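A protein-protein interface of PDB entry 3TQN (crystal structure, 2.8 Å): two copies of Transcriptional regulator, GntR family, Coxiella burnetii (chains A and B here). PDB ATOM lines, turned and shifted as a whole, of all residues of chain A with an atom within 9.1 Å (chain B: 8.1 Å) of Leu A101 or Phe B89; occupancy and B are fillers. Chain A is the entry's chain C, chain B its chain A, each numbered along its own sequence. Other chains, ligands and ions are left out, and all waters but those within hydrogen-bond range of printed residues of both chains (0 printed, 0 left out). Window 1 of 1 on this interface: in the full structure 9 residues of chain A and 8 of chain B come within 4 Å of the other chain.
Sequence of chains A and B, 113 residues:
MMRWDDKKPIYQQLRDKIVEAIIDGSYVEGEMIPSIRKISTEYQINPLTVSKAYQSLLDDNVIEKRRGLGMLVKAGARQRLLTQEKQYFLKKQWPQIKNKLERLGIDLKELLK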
ATOM      1  N   TRP A  94      -0.883 -15.036 -24.287  1.00  0.00           N
ATOM      2  CA  TRP A  94      -1.216 -15.679 -23.019  1.00  0.00           C
ATOM      3  C   TRP A  94      -1.213 -17.207 -23.101  1.00  0.00           C
ATOM      4  O   TRP A  94      -0.703 -17.873 -22.197  1.00  0.00           O
ATOM      5  CB  TRP A  94      -2.552 -15.164 -22.485  1.00  0.00           C
ATOM      6  CG  TRP A  94      -3.068 -15.942 -21.322  1.00  0.00           C
ATOM      7  CD1 TRP A  94      -4.305 -16.500 -21.195  1.00  0.00           C
ATOM      8  CD2 TRP A  94      -2.355 -16.270 -20.122  1.00  0.00           C
ATOM      9  NE1 TRP A  94      -4.412 -17.145 -19.987  1.00  0.00           N
ATOM     10  CE2 TRP A  94      -3.226 -17.019 -19.310  1.00  0.00           C
ATOM     11  CE3 TRP A  94      -1.064 -15.997 -19.654  1.00  0.00           C
ATOM     12  CZ2 TRP A  94      -2.853 -17.501 -18.058  1.00  0.00           C
ATOM     13  CZ3 TRP A  94      -0.694 -16.477 -18.410  1.00  0.00           C
ATOM     14  CH2 TRP A  94      -1.586 -17.220 -17.626  1.00  0.00           C
ATOM     15  N   PRO A  95      -1.790 -17.775 -24.174  1.00  0.00           N
ATOM     16  CA  PRO A  95      -1.589 -19.221 -24.300  1.00  0.00           C
ATOM     17  C   PRO A  95      -0.151 -19.528 -24.727  1.00  0.00           C
ATOM     18  O   PRO A  95       0.620 -18.610 -24.981  1.00  0.00           O
ATOM     19  CB  PRO A  95      -2.595 -19.628 -25.382  1.00  0.00           C
ATOM     20  CG  PRO A  95      -2.831 -18.389 -26.167  1.00  0.00           C
ATOM     21  CD  PRO A  95      -2.719 -17.248 -25.189  1.00  0.00           C
ATOM     22  N   GLN A  96       0.189 -20.807 -24.813  1.00  0.00           N
ATOM     23  CA  GLN A  96       1.561 -21.265 -25.007  1.00  0.00           C
ATOM     24  C   GLN A  96       2.395 -21.008 -23.749  1.00  0.00           C
ATOM     25  O   GLN A  96       3.460 -21.603 -23.573  1.00  0.00           O
ATOM     26  CB  GLN A  96       2.200 -20.560 -26.209  1.00  0.00           C
ATOM     27  CG  GLN A  96       1.318 -20.518 -27.449  1.00  0.00           C
ATOM     28  CD  GLN A  96       1.073 -19.102 -27.943  1.00  0.00           C
ATOM     29  OE1 GLN A  96       2.006 -18.390 -28.316  1.00  0.00           O
ATOM     30  NE2 GLN A  96      -0.187 -18.684 -27.938  1.00  0.00           N
ATOM     31  N   ILE A  97       1.908 -20.119 -22.883  1.00  0.00           N
ATOM     32  CA  ILE A  97       2.477 -19.921 -21.550  1.00  0.00           C
ATOM     33  C   ILE A  97       1.643 -20.582 -20.435  1.00  0.00           C
ATOM     34  O   ILE A  97       2.014 -20.520 -19.264  1.00  0.00           O
ATOM     35  CB  ILE A  97       2.653 -18.417 -21.196  1.00  0.00           C
ATOM     36  CG1 ILE A  97       2.276 -17.526 -22.377  1.00  0.00           C
ATOM     37  CG2 ILE A  97       4.092 -18.136 -20.756  1.00  0.00           C
ATOM     38  CD1 ILE A  97       2.387 -16.035 -22.072  1.00  0.00           C
ATOM     39  N   LYS A  98       0.523 -21.206 -20.791  1.00  0.00           N
ATOM     40  CA  LYS A  98      -0.559 -21.449 -19.821  1.00  0.00           C
ATOM     41  C   LYS A  98      -0.582 -22.668 -18.850  1.00  0.00           C
ATOM     42  O   LYS A  98      -0.677 -22.459 -17.646  1.00  0.00           O
ATOM     43  CB  LYS A  98      -1.951 -21.264 -20.453  1.00  0.00           C
ATOM     44  CG  LYS A  98      -3.029 -21.149 -19.383  1.00  0.00           C
ATOM     45  CD  LYS A  98      -4.429 -21.342 -19.933  1.00  0.00           C
ATOM     46  CE  LYS A  98      -5.324 -21.896 -18.836  1.00  0.00           C
ATOM     47  NZ  LYS A  98      -6.773 -21.821 -19.163  1.00  0.00           N
ATOM     48  N   ASN A  99      -0.599 -23.914 -19.333  1.00  0.00           N
ATOM     49  CA  ASN A  99      -0.203 -24.282 -20.694  1.00  0.00           C
ATOM     50  C   ASN A  99       1.273 -23.985 -20.988  1.00  0.00           C
ATOM     51  O   ASN A  99       1.638 -23.048 -21.689  1.00  0.00           O
ATOM     52  CB  ASN A  99      -1.212 -23.780 -21.740  1.00  0.00           C
ATOM     53  CG  ASN A  99      -0.564 -23.088 -22.897  1.00  0.00           C
ATOM     54  OD1 ASN A  99      -0.589 -21.862 -22.996  1.00  0.00           O
ATOM     55  ND2 ASN A  99       0.043 -23.867 -23.779  1.00  0.00           N
ATOM     56  N   LYS A 100       2.103 -24.838 -20.399  1.00  0.00           N
ATOM     57  CA  LYS A 100       3.533 -24.617 -20.196  1.00  0.00           C
ATOM     58  C   LYS A 100       3.806 -23.931 -18.848  1.00  0.00           C
ATOM     59  O   LYS A 100       4.960 -23.833 -18.430  1.00  0.00           O
ATOM     60  CB  LYS A 100       4.167 -23.863 -21.376  1.00  0.00           C
ATOM     61  CG  LYS A 100       5.657 -23.631 -21.248  1.00  0.00           C
ATOM     62  CD  LYS A 100       5.939 -22.183 -20.888  1.00  0.00           C
ATOM     63  CE  LYS A 100       7.311 -22.020 -20.248  1.00  0.00           C
ATOM     64  NZ  LYS A 100       8.420 -22.094 -21.238  1.00  0.00           N
ATOM     65  N   LEU A 101       2.760 -23.464 -18.165  1.00  0.00           N
ATOM     66  CA  LEU A 101       2.827 -23.308 -16.707  1.00  0.00           C
ATOM     67  C   LEU A 101       2.482 -24.661 -16.096  1.00  0.00           C
ATOM     68  O   LEU A 101       3.118 -25.123 -15.152  1.00  0.00           O
ATOM     69  CB  LEU A 101       1.869 -22.227 -16.193  1.00  0.00           C
ATOM     70  CG  LEU A 101       2.379 -20.781 -16.099  1.00  0.00           C
ATOM     71  CD1 LEU A 101       1.233 -19.779 -16.228  1.00  0.00           C
ATOM     72  CD2 LEU A 101       3.161 -20.541 -14.812  1.00  0.00           C
ATOM     73  N   GLU A 102       1.461 -25.289 -16.676  1.00  0.00           N
ATOM     74  CA  GLU A 102       0.985 -26.608 -16.276  1.00  0.00           C
ATOM     75  C   GLU A 102       2.016 -27.689 -16.588  1.00  0.00           C
ATOM     76  O   GLU A 102       2.152 -28.663 -15.843  1.00  0.00           O
ATOM     77  CB  GLU A 102      -0.344 -26.922 -16.979  1.00  0.00           C
ATOM     78  CG  GLU A 102      -0.267 -26.953 -18.510  1.00  0.00           C
ATOM     79  CD  GLU A 102      -1.635 -26.906 -19.178  1.00  0.00           C
ATOM     80  OE1 GLU A 102      -2.640 -26.690 -18.466  1.00  0.00           O
ATOM     81  OE2 GLU A 102      -1.704 -27.078 -20.414  1.00  0.00           O
ATOM     82  N   ARG A 103       2.740 -27.511 -17.689  1.00  0.00           N
ATOM     83  CA  ARG A 103       3.784 -28.447 -18.077  1.00  0.00           C
ATOM     84  C   ARG A 103       4.830 -28.545 -16.974  1.00  0.00           C
ATOM     85  O   ARG A 103       5.402 -29.612 -16.762  1.00  0.00           O
ATOM     86  CB  ARG A 103       4.451 -28.016 -19.390  1.00  0.00           C
ATOM     87  CG  ARG A 103       5.642 -28.883 -19.791  1.00  0.00           C
ATOM     88  CD  ARG A 103       6.184 -28.523 -21.170  1.00  0.00           C
ATOM     89  NE  ARG A 103       7.313 -27.595 -21.110  1.00  0.00           N
ATOM     90  CZ  ARG A 103       8.555 -27.953 -20.796  1.00  0.00           C
ATOM     91  NH1 ARG A 103       8.827 -29.216 -20.498  1.00  0.00           N
ATOM     92  NH2 ARG A 103       9.522 -27.046 -20.769  1.00  0.00           N
ATOM     93  N   LEU A 104       5.060 -27.444 -16.258  1.00  0.00           N
ATOM     94  CA  LEU A 104       6.140 -27.388 -15.265  1.00  0.00           C
ATOM     95  C   LEU A 104       5.686 -27.272 -13.795  1.00  0.00           C
ATOM     96  O   LEU A 104       5.599 -28.286 -13.096  1.00  0.00           O
ATOM     97  CB  LEU A 104       7.017 -26.173 -15.575  1.00  0.00           C
ATOM     98  CG  LEU A 104       7.344 -25.946 -17.050  1.00  0.00           C
ATOM     99  CD1 LEU A 104       7.785 -24.513 -17.282  1.00  0.00           C
ATOM    100  CD2 LEU A 104       8.405 -26.932 -17.502  1.00  0.00           C
ATOM    101  N   GLY A 105       5.326 -26.050 -13.376  1.00  0.00           N
ATOM    102  CA  GLY A 105       4.824 -25.755 -12.039  1.00  0.00           C
ATOM    103  C   GLY A 105       3.782 -24.652 -12.067  1.00  0.00           C
ATOM    104  O   GLY A 105       3.768 -23.809 -12.965  1.00  0.00           O
ATOM    105  N   ILE A 106       2.929 -24.618 -11.048  1.00  0.00           N
ATOM    106  CA  ILE A 106       1.686 -23.847 -11.166  1.00  0.00           C
ATOM    107  C   ILE A 106       1.132 -23.329  -9.837  1.00  0.00           C
ATOM    108  O   ILE A 106       1.788 -23.424  -8.801  1.00  0.00           O
ATOM    109  CB  ILE A 106       0.597 -24.668 -11.928  1.00  0.00           C
ATOM    110  CG1 ILE A 106      -0.647 -23.813 -12.207  1.00  0.00           C
ATOM    111  CG2 ILE A 106       0.244 -25.943 -11.138  1.00  0.00           C
ATOM    112  CD1 ILE A 106      -0.442 -22.732 -13.225  1.00  0.00           C
ATOM    113  N   ASP A 107      -0.080 -22.783  -9.886  1.00  0.00           N
ATOM    114  CA  ASP A 107      -0.725 -22.221  -8.713  1.00  0.00           C
ATOM    115  C   ASP A 107       0.082 -21.080  -8.102  1.00  0.00           C
ATOM    116  O   ASP A 107       0.719 -21.258  -7.070  1.00  0.00           O
ATOM    117  CB  ASP A 107      -1.011 -23.304  -7.669  1.00  0.00           C
ATOM    118  CG  ASP A 107      -2.482 -23.674  -7.601  1.00  0.00           C
ATOM    119  OD1 ASP A 107      -2.799 -24.797  -7.155  1.00  0.00           O
ATOM    120  OD2 ASP A 107      -3.319 -22.844  -8.000  1.00  0.00           O
ATOM    121  N   LEU A 108       0.065 -19.912  -8.743  1.00  0.00           N
ATOM    122  CA  LEU A 108       0.936 -18.813  -8.325  1.00  0.00           C
ATOM    123  C   LEU A 108       0.845 -18.634  -6.813  1.00  0.00           C
ATOM    124  O   LEU A 108      -0.230 -18.735  -6.226  1.00  0.00           O
ATOM    125  CB  LEU A 108       0.617 -17.510  -9.063  1.00  0.00           C
ATOM    126  CG  LEU A 108       1.634 -16.381  -8.900  1.00  0.00           C
ATOM    127  CD1 LEU A 108       1.249 -15.471  -7.744  1.00  0.00           C
ATOM    128  CD2 LEU A 108       3.033 -16.958  -8.714  1.00  0.00           C
ATOM    129  N   LYS A 109       1.984 -18.356  -6.194  1.00  0.00           N
ATOM    130  CA  LYS A 109       2.209 -18.717  -4.807  1.00  0.00           C
ATOM    131  C   LYS A 109       2.848 -17.598  -4.003  1.00  0.00           C
ATOM    132  O   LYS A 109       3.503 -16.720  -4.556  1.00  0.00           O
ATOM    133  CB  LYS A 109       3.134 -19.933  -4.833  1.00  0.00           C
ATOM    134  CG  LYS A 109       4.039 -19.877  -6.054  1.00  0.00           C
ATOM    135  CD  LYS A 109       4.636 -21.213  -6.408  1.00  0.00           C
ATOM    136  CE  LYS A 109       3.889 -21.869  -7.550  1.00  0.00           C
ATOM    137  NZ  LYS A 109       4.410 -23.240  -7.790  1.00  0.00           N
ATOM    138  N   LEU B  82      14.130 -30.995 -14.754  1.00  0.00           N
ATOM    139  CA  LEU B  82      12.760 -30.502 -14.642  1.00  0.00           C
ATOM    140  C   LEU B  82      12.658 -29.384 -13.610  1.00  0.00           C
ATOM    141  O   LEU B  82      12.029 -28.354 -13.860  1.00  0.00           O
ATOM    142  CB  LEU B  82      11.804 -31.645 -14.292  1.00  0.00           C
ATOM    143  CG  LEU B  82      11.568 -32.668 -15.405  1.00  0.00           C
ATOM    144  CD1 LEU B  82      10.987 -33.963 -14.851  1.00  0.00           C
ATOM    145  CD2 LEU B  82      10.668 -32.085 -16.485  1.00  0.00           C
ATOM    146  N   THR B  83      13.279 -29.590 -12.452  1.00  0.00           N
ATOM    147  CA  THR B  83      13.303 -28.570 -11.410  1.00  0.00           C
ATOM    148  C   THR B  83      14.052 -27.333 -11.891  1.00  0.00           C
ATOM    149  O   THR B  83      13.641 -26.205 -11.620  1.00  0.00           O
ATOM    150  CB  THR B  83      13.953 -29.089 -10.114  1.00  0.00           C
ATOM    151  OG1 THR B  83      15.309 -29.471 -10.376  1.00  0.00           O
ATOM    152  CG2 THR B  83      13.185 -30.286  -9.577  1.00  0.00           C
ATOM    153  N   GLN B  84      15.155 -27.553 -12.603  1.00  0.00           N
ATOM    154  CA  GLN B  84      15.921 -26.455 -13.183  1.00  0.00           C
ATOM    155  C   GLN B  84      15.067 -25.632 -14.139  1.00  0.00           C
ATOM    156  O   GLN B  84      15.047 -24.404 -14.060  1.00  0.00           O
ATOM    157  CB  GLN B  84      17.161 -26.975 -13.913  1.00  0.00           C
ATOM    158  CG  GLN B  84      18.373 -27.187 -13.022  1.00  0.00           C
ATOM    159  CD  GLN B  84      19.629 -27.480 -13.818  1.00  0.00           C
ATOM    160  OE1 GLN B  84      20.284 -28.502 -13.613  1.00  0.00           O
ATOM    161  NE2 GLN B  84      19.972 -26.580 -14.732  1.00  0.00           N
ATOM    162  N   GLU B  85      14.372 -26.309 -15.048  1.00  0.00           N
ATOM    163  CA  GLU B  85      13.504 -25.621 -15.994  1.00  0.00           C
ATOM    164  C   GLU B  85      12.487 -24.784 -15.235  1.00  0.00           C
ATOM    165  O   GLU B  85      12.287 -23.607 -15.533  1.00  0.00           O
ATOM    166  CB  GLU B  85      12.788 -26.617 -16.910  1.00  0.00           C
ATOM    167  CG  GLU B  85      13.710 -27.391 -17.836  1.00  0.00           C
ATOM    168  CD  GLU B  85      12.958 -28.105 -18.946  1.00  0.00           C
ATOM    169  OE1 GLU B  85      11.783 -28.472 -18.733  1.00  0.00           O
ATOM    170  OE2 GLU B  85      13.543 -28.289 -20.034  1.00  0.00           O
ATOM    171  N   LYS B  86      11.855 -25.401 -14.242  1.00  0.00           N
ATOM    172  CA  LYS B  86      10.858 -24.718 -13.432  1.00  0.00           C
ATOM    173  C   LYS B  86      11.463 -23.480 -12.771  1.00  0.00           C
ATOM    174  O   LYS B  86      10.925 -22.381 -12.891  1.00  0.00           O
ATOM    175  CB  LYS B  86      10.291 -25.667 -12.371  1.00  0.00           C
ATOM    176  CG  LYS B  86       8.836 -25.400 -12.021  1.00  0.00           C
ATOM    177  CD  LYS B  86       8.497 -25.877 -10.616  1.00  0.00           C
ATOM    178  CE  LYS B  86       7.495 -27.019 -10.631  1.00  0.00           C
ATOM    179  NZ  LYS B  86       6.915 -27.256  -9.280  1.00  0.00           N
ATOM    180  N   GLN B  87      12.590 -23.665 -12.089  1.00  0.00           N
ATOM    181  CA  GLN B  87      13.274 -22.569 -11.404  1.00  0.00           C
ATOM    182  C   GLN B  87      13.674 -21.438 -12.348  1.00  0.00           C
ATOM    183  O   GLN B  87      13.406 -20.269 -12.070  1.00  0.00           O
ATOM    184  CB  GLN B  87      14.510 -23.080 -10.657  1.00  0.00           C
ATOM    185  CG  GLN B  87      14.203 -23.966  -9.460  1.00  0.00           C
ATOM    186  CD  GLN B  87      15.425 -24.211  -8.596  1.00  0.00           C
ATOM    187  OE1 GLN B  87      16.499 -23.665  -8.853  1.00  0.00           O
ATOM    188  NE2 GLN B  87      15.266 -25.029  -7.563  1.00  0.00           N
ATOM    189  N   TYR B  88      14.325 -21.784 -13.455  1.00  0.00           N
ATOM    190  CA  TYR B  88      14.736 -20.781 -14.432  1.00  0.00           C
ATOM    191  C   TYR B  88      13.539 -19.967 -14.908  1.00  0.00           C
ATOM    192  O   TYR B  88      13.627 -18.749 -15.042  1.00  0.00           O
ATOM    193  CB  TYR B  88      15.446 -21.425 -15.626  1.00  0.00           C
ATOM    194  CG  TYR B  88      15.740 -20.451 -16.747  1.00  0.00           C
ATOM    195  CD1 TYR B  88      16.810 -19.570 -16.665  1.00  0.00           C
ATOM    196  CD2 TYR B  88      14.945 -20.410 -17.884  1.00  0.00           C
ATOM    197  CE1 TYR B  88      17.081 -18.675 -17.688  1.00  0.00           C
ATOM    198  CE2 TYR B  88      15.209 -19.520 -18.911  1.00  0.00           C
ATOM    199  CZ  TYR B  88      16.278 -18.656 -18.807  1.00  0.00           C
ATOM    200  OH  TYR B  88      16.544 -17.768 -19.826  1.00  0.00           O
ATOM    201  N   PHE B  89      12.424 -20.643 -15.166  1.00  0.00           N
ATOM    202  CA  PHE B  89      11.209 -19.955 -15.580  1.00  0.00           C
ATOM    203  C   PHE B  89      10.741 -18.996 -14.489  1.00  0.00           C
ATOM    204  O   PHE B  89      10.447 -17.834 -14.758  1.00  0.00           O
ATOM    205  CB  PHE B  89      10.103 -20.957 -15.927  1.00  0.00           C
ATOM    206  CG  PHE B  89       8.762 -20.320 -16.172  1.00  0.00           C
ATOM    207  CD1 PHE B  89       8.536 -19.564 -17.310  1.00  0.00           C
ATOM    208  CD2 PHE B  89       7.727 -20.480 -15.265  1.00  0.00           C
ATOM    209  CE1 PHE B  89       7.304 -18.975 -17.537  1.00  0.00           C
ATOM    210  CE2 PHE B  89       6.492 -19.894 -15.488  1.00  0.00           C
ATOM    211  CZ  PHE B  89       6.281 -19.141 -16.626  1.00  0.00           C
ATOM    212  N   LEU B  90      10.697 -19.486 -13.254  1.00  0.00           N
ATOM    213  CA  LEU B  90      10.207 -18.696 -12.129  1.00  0.00           C
ATOM    214  C   LEU B  90      10.953 -17.377 -11.927  1.00  0.00           C
ATOM    215  O   LEU B  90      10.344 -16.311 -11.949  1.00  0.00           O
ATOM    216  CB  LEU B  90      10.238 -19.518 -10.835  1.00  0.00           C
ATOM    217  CG  LEU B  90       9.194 -20.627 -10.696  1.00  0.00           C
ATOM    218  CD1 LEU B  90       9.179 -21.158  -9.273  1.00  0.00           C
ATOM    219  CD2 LEU B  90       7.819 -20.109 -11.083  1.00  0.00           C
ATOM    220  N   LYS B  91      12.266 -17.445 -11.729  1.00  0.00           N
ATOM    221  CA  LYS B  91      13.053 -16.244 -11.449  1.00  0.00           C
ATOM    222  C   LYS B  91      13.382 -15.401 -12.680  1.00  0.00           C
ATOM    223  O   LYS B  91      13.204 -14.182 -12.668  1.00  0.00           O
ATOM    224  CB  LYS B  91      14.345 -16.603 -10.714  1.00  0.00           C
ATOM    225  CG  LYS B  91      14.127 -17.204  -9.342  1.00  0.00           C
ATOM    226  CD  LYS B  91      15.424 -17.668  -8.718  1.00  0.00           C
ATOM    227  CE  LYS B  91      15.144 -18.481  -7.474  1.00  0.00           C
ATOM    228  NZ  LYS B  91      14.240 -19.613  -7.801  1.00  0.00           N
ATOM    229  N   LYS B  92      13.848 -16.049 -13.744  1.00  0.00           N
ATOM    230  CA  LYS B  92      14.324 -15.325 -14.923  1.00  0.00           C
ATOM    231  C   LYS B  92      13.283 -15.084 -16.019  1.00  0.00           C
ATOM    232  O   LYS B  92      13.572 -14.425 -17.016  1.00  0.00           O
ATOM    233  CB  LYS B  92      15.572 -15.999 -15.515  1.00  0.00           C
ATOM    234  CG  LYS B  92      16.848 -15.555 -14.832  1.00  0.00           C
ATOM    235  CD  LYS B  92      16.715 -14.087 -14.452  1.00  0.00           C
ATOM    236  CE  LYS B  92      18.044 -13.454 -14.085  1.00  0.00           C
ATOM    237  NZ  LYS B  92      17.868 -11.997 -13.827  1.00  0.00           N
ATOM    238  N   GLN B  93      12.075 -15.602 -15.834  1.00  0.00           N
ATOM    239  CA  GLN B  93      11.028 -15.426 -16.839  1.00  0.00           C
ATOM    240  C   GLN B  93       9.731 -14.850 -16.281  1.00  0.00           C
ATOM    241  O   GLN B  93       9.307 -13.768 -16.678  1.00  0.00           O
ATOM    242  CB  GLN B  93      10.736 -16.739 -17.570  1.00  0.00           C
ATOM    243  CG  GLN B  93      11.788 -17.151 -18.580  1.00  0.00           C
ATOM    244  CD  GLN B  93      11.239 -18.127 -19.599  1.00  0.00           C
ATOM    245  OE1 GLN B  93      10.257 -17.836 -20.284  1.00  0.00           O
ATOM    246  NE2 GLN B  93      11.861 -19.295 -19.699  1.00  0.00           N
ATOM    247  N   TRP B  94       9.101 -15.590 -15.373  1.00  0.00           N
ATOM    248  CA  TRP B  94       7.777 -15.237 -14.866  1.00  0.00           C
ATOM    249  C   TRP B  94       7.613 -13.746 -14.563  1.00  0.00           C
ATOM    250  O   TRP B  94       6.653 -13.126 -15.020  1.00  0.00           O
ATOM    251  CB  TRP B  94       7.425 -16.090 -13.646  1.00  0.00           C
ATOM    252  CG  TRP B  94       6.162 -15.667 -12.978  1.00  0.00           C
ATOM    253  CD1 TRP B  94       6.023 -15.231 -11.693  1.00  0.00           C
ATOM    254  CD2 TRP B  94       4.857 -15.619 -13.564  1.00  0.00           C
ATOM    255  NE1 TRP B  94       4.708 -14.924 -11.439  1.00  0.00           N
ATOM    256  CE2 TRP B  94       3.972 -15.153 -12.571  1.00  0.00           C
ATOM    257  CE3 TRP B  94       4.349 -15.930 -14.830  1.00  0.00           C
ATOM    258  CZ2 TRP B  94       2.610 -14.991 -12.805  1.00  0.00           C
ATOM    259  CZ3 TRP B  94       2.995 -15.767 -15.057  1.00  0.00           C
ATOM    260  CH2 TRP B  94       2.141 -15.301 -14.051  1.00  0.00           C
ATOM    261  N   PRO B  95       8.543 -13.162 -13.793  1.00  0.00           N
ATOM    262  CA  PRO B  95       8.496 -11.703 -13.662  1.00  0.00           C
ATOM    263  C   PRO B  95       8.987 -11.067 -14.965  1.00  0.00           C
ATOM    264  O   PRO B  95       9.816 -11.671 -15.643  1.00  0.00           O
ATOM    265  CB  PRO B  95       9.466 -11.426 -12.508  1.00  0.00           C
ATOM    266  CG  PRO B  95      10.430 -12.559 -12.559  1.00  0.00           C
ATOM    267  CD  PRO B  95       9.633 -13.757 -13.002  1.00  0.00           C
ATOM    268  N   ILE B  97       6.950 -10.801 -17.212  1.00  0.00           N
ATOM    269  CA  ILE B  97       5.647 -11.102 -17.797  1.00  0.00           C
ATOM    270  C   ILE B  97       4.604 -10.649 -16.779  1.00  0.00           C
ATOM    271  O   ILE B  97       3.402 -10.730 -17.009  1.00  0.00           O
ATOM    272  CB  ILE B  97       5.481 -12.614 -18.144  1.00  0.00           C
ATOM    273  CG1 ILE B  97       4.532 -13.318 -17.167  1.00  0.00           C
ATOM    274  CG2 ILE B  97       6.829 -13.312 -18.200  1.00  0.00           C
ATOM    275  CD1 ILE B  97       3.181 -13.661 -17.763  1.00  0.00           C
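Leu A101 touches Phe B89 (CD2 to CE2, 3.5 Å).
CD2 of Leu A104 touches OE1 of Glu B85, 3.9 Å away.
Lys B86 touches Leu A104 (CE to O, 3.4 Å).
CA of Gly A105 touches CE of Lys B86, 3.3 Å away.
Leu A108 touches Trp B94 (CD2 to NE1, 3.8 Å).
Positions printed for both chains: 94, 95 and 97.
The backbone NH (N) of Trp B94 is in hydrogen-bond range of the backbone carbonyl oxygen (O) of Phe B89, 2.7 Å away.
Leu A101 touches one residue of chain B.
Printed residues of chain B within 4 Å of Arg A103: Glu B85.
Of the printed residues of chain B, Leu A104 touches Glu B85 (3.9 Å) and Lys B86 (3.4 Å).
Of the printed residues of chain B, Leu A108 touches Trp B94 (3.8 Å).
Of chain A, only Leu A101 comes within 4 Å of Phe B89.
Lys B91 touches none of the printed residues of chain A.
No residue of chain A comes within 4 Å of Gln B93.
The nearest residue of chain B that does not touch Leu A101 is Trp B94 (4.5 Å).
The nearest residue of chain A that does not touch Phe B89 is Lys A100 (4.02 Å).
Of the 16 printed residues of chain A, 5 touch a printed residue of chain B.
Of the 15 printed residues of chain B, 4 touch a printed residue of chain A.
The guanidinium group (NH2) of Arg A103 is in salt-bridge range of the side-chain carboxylate (OE1) of Glu B85 (3.4 Å).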
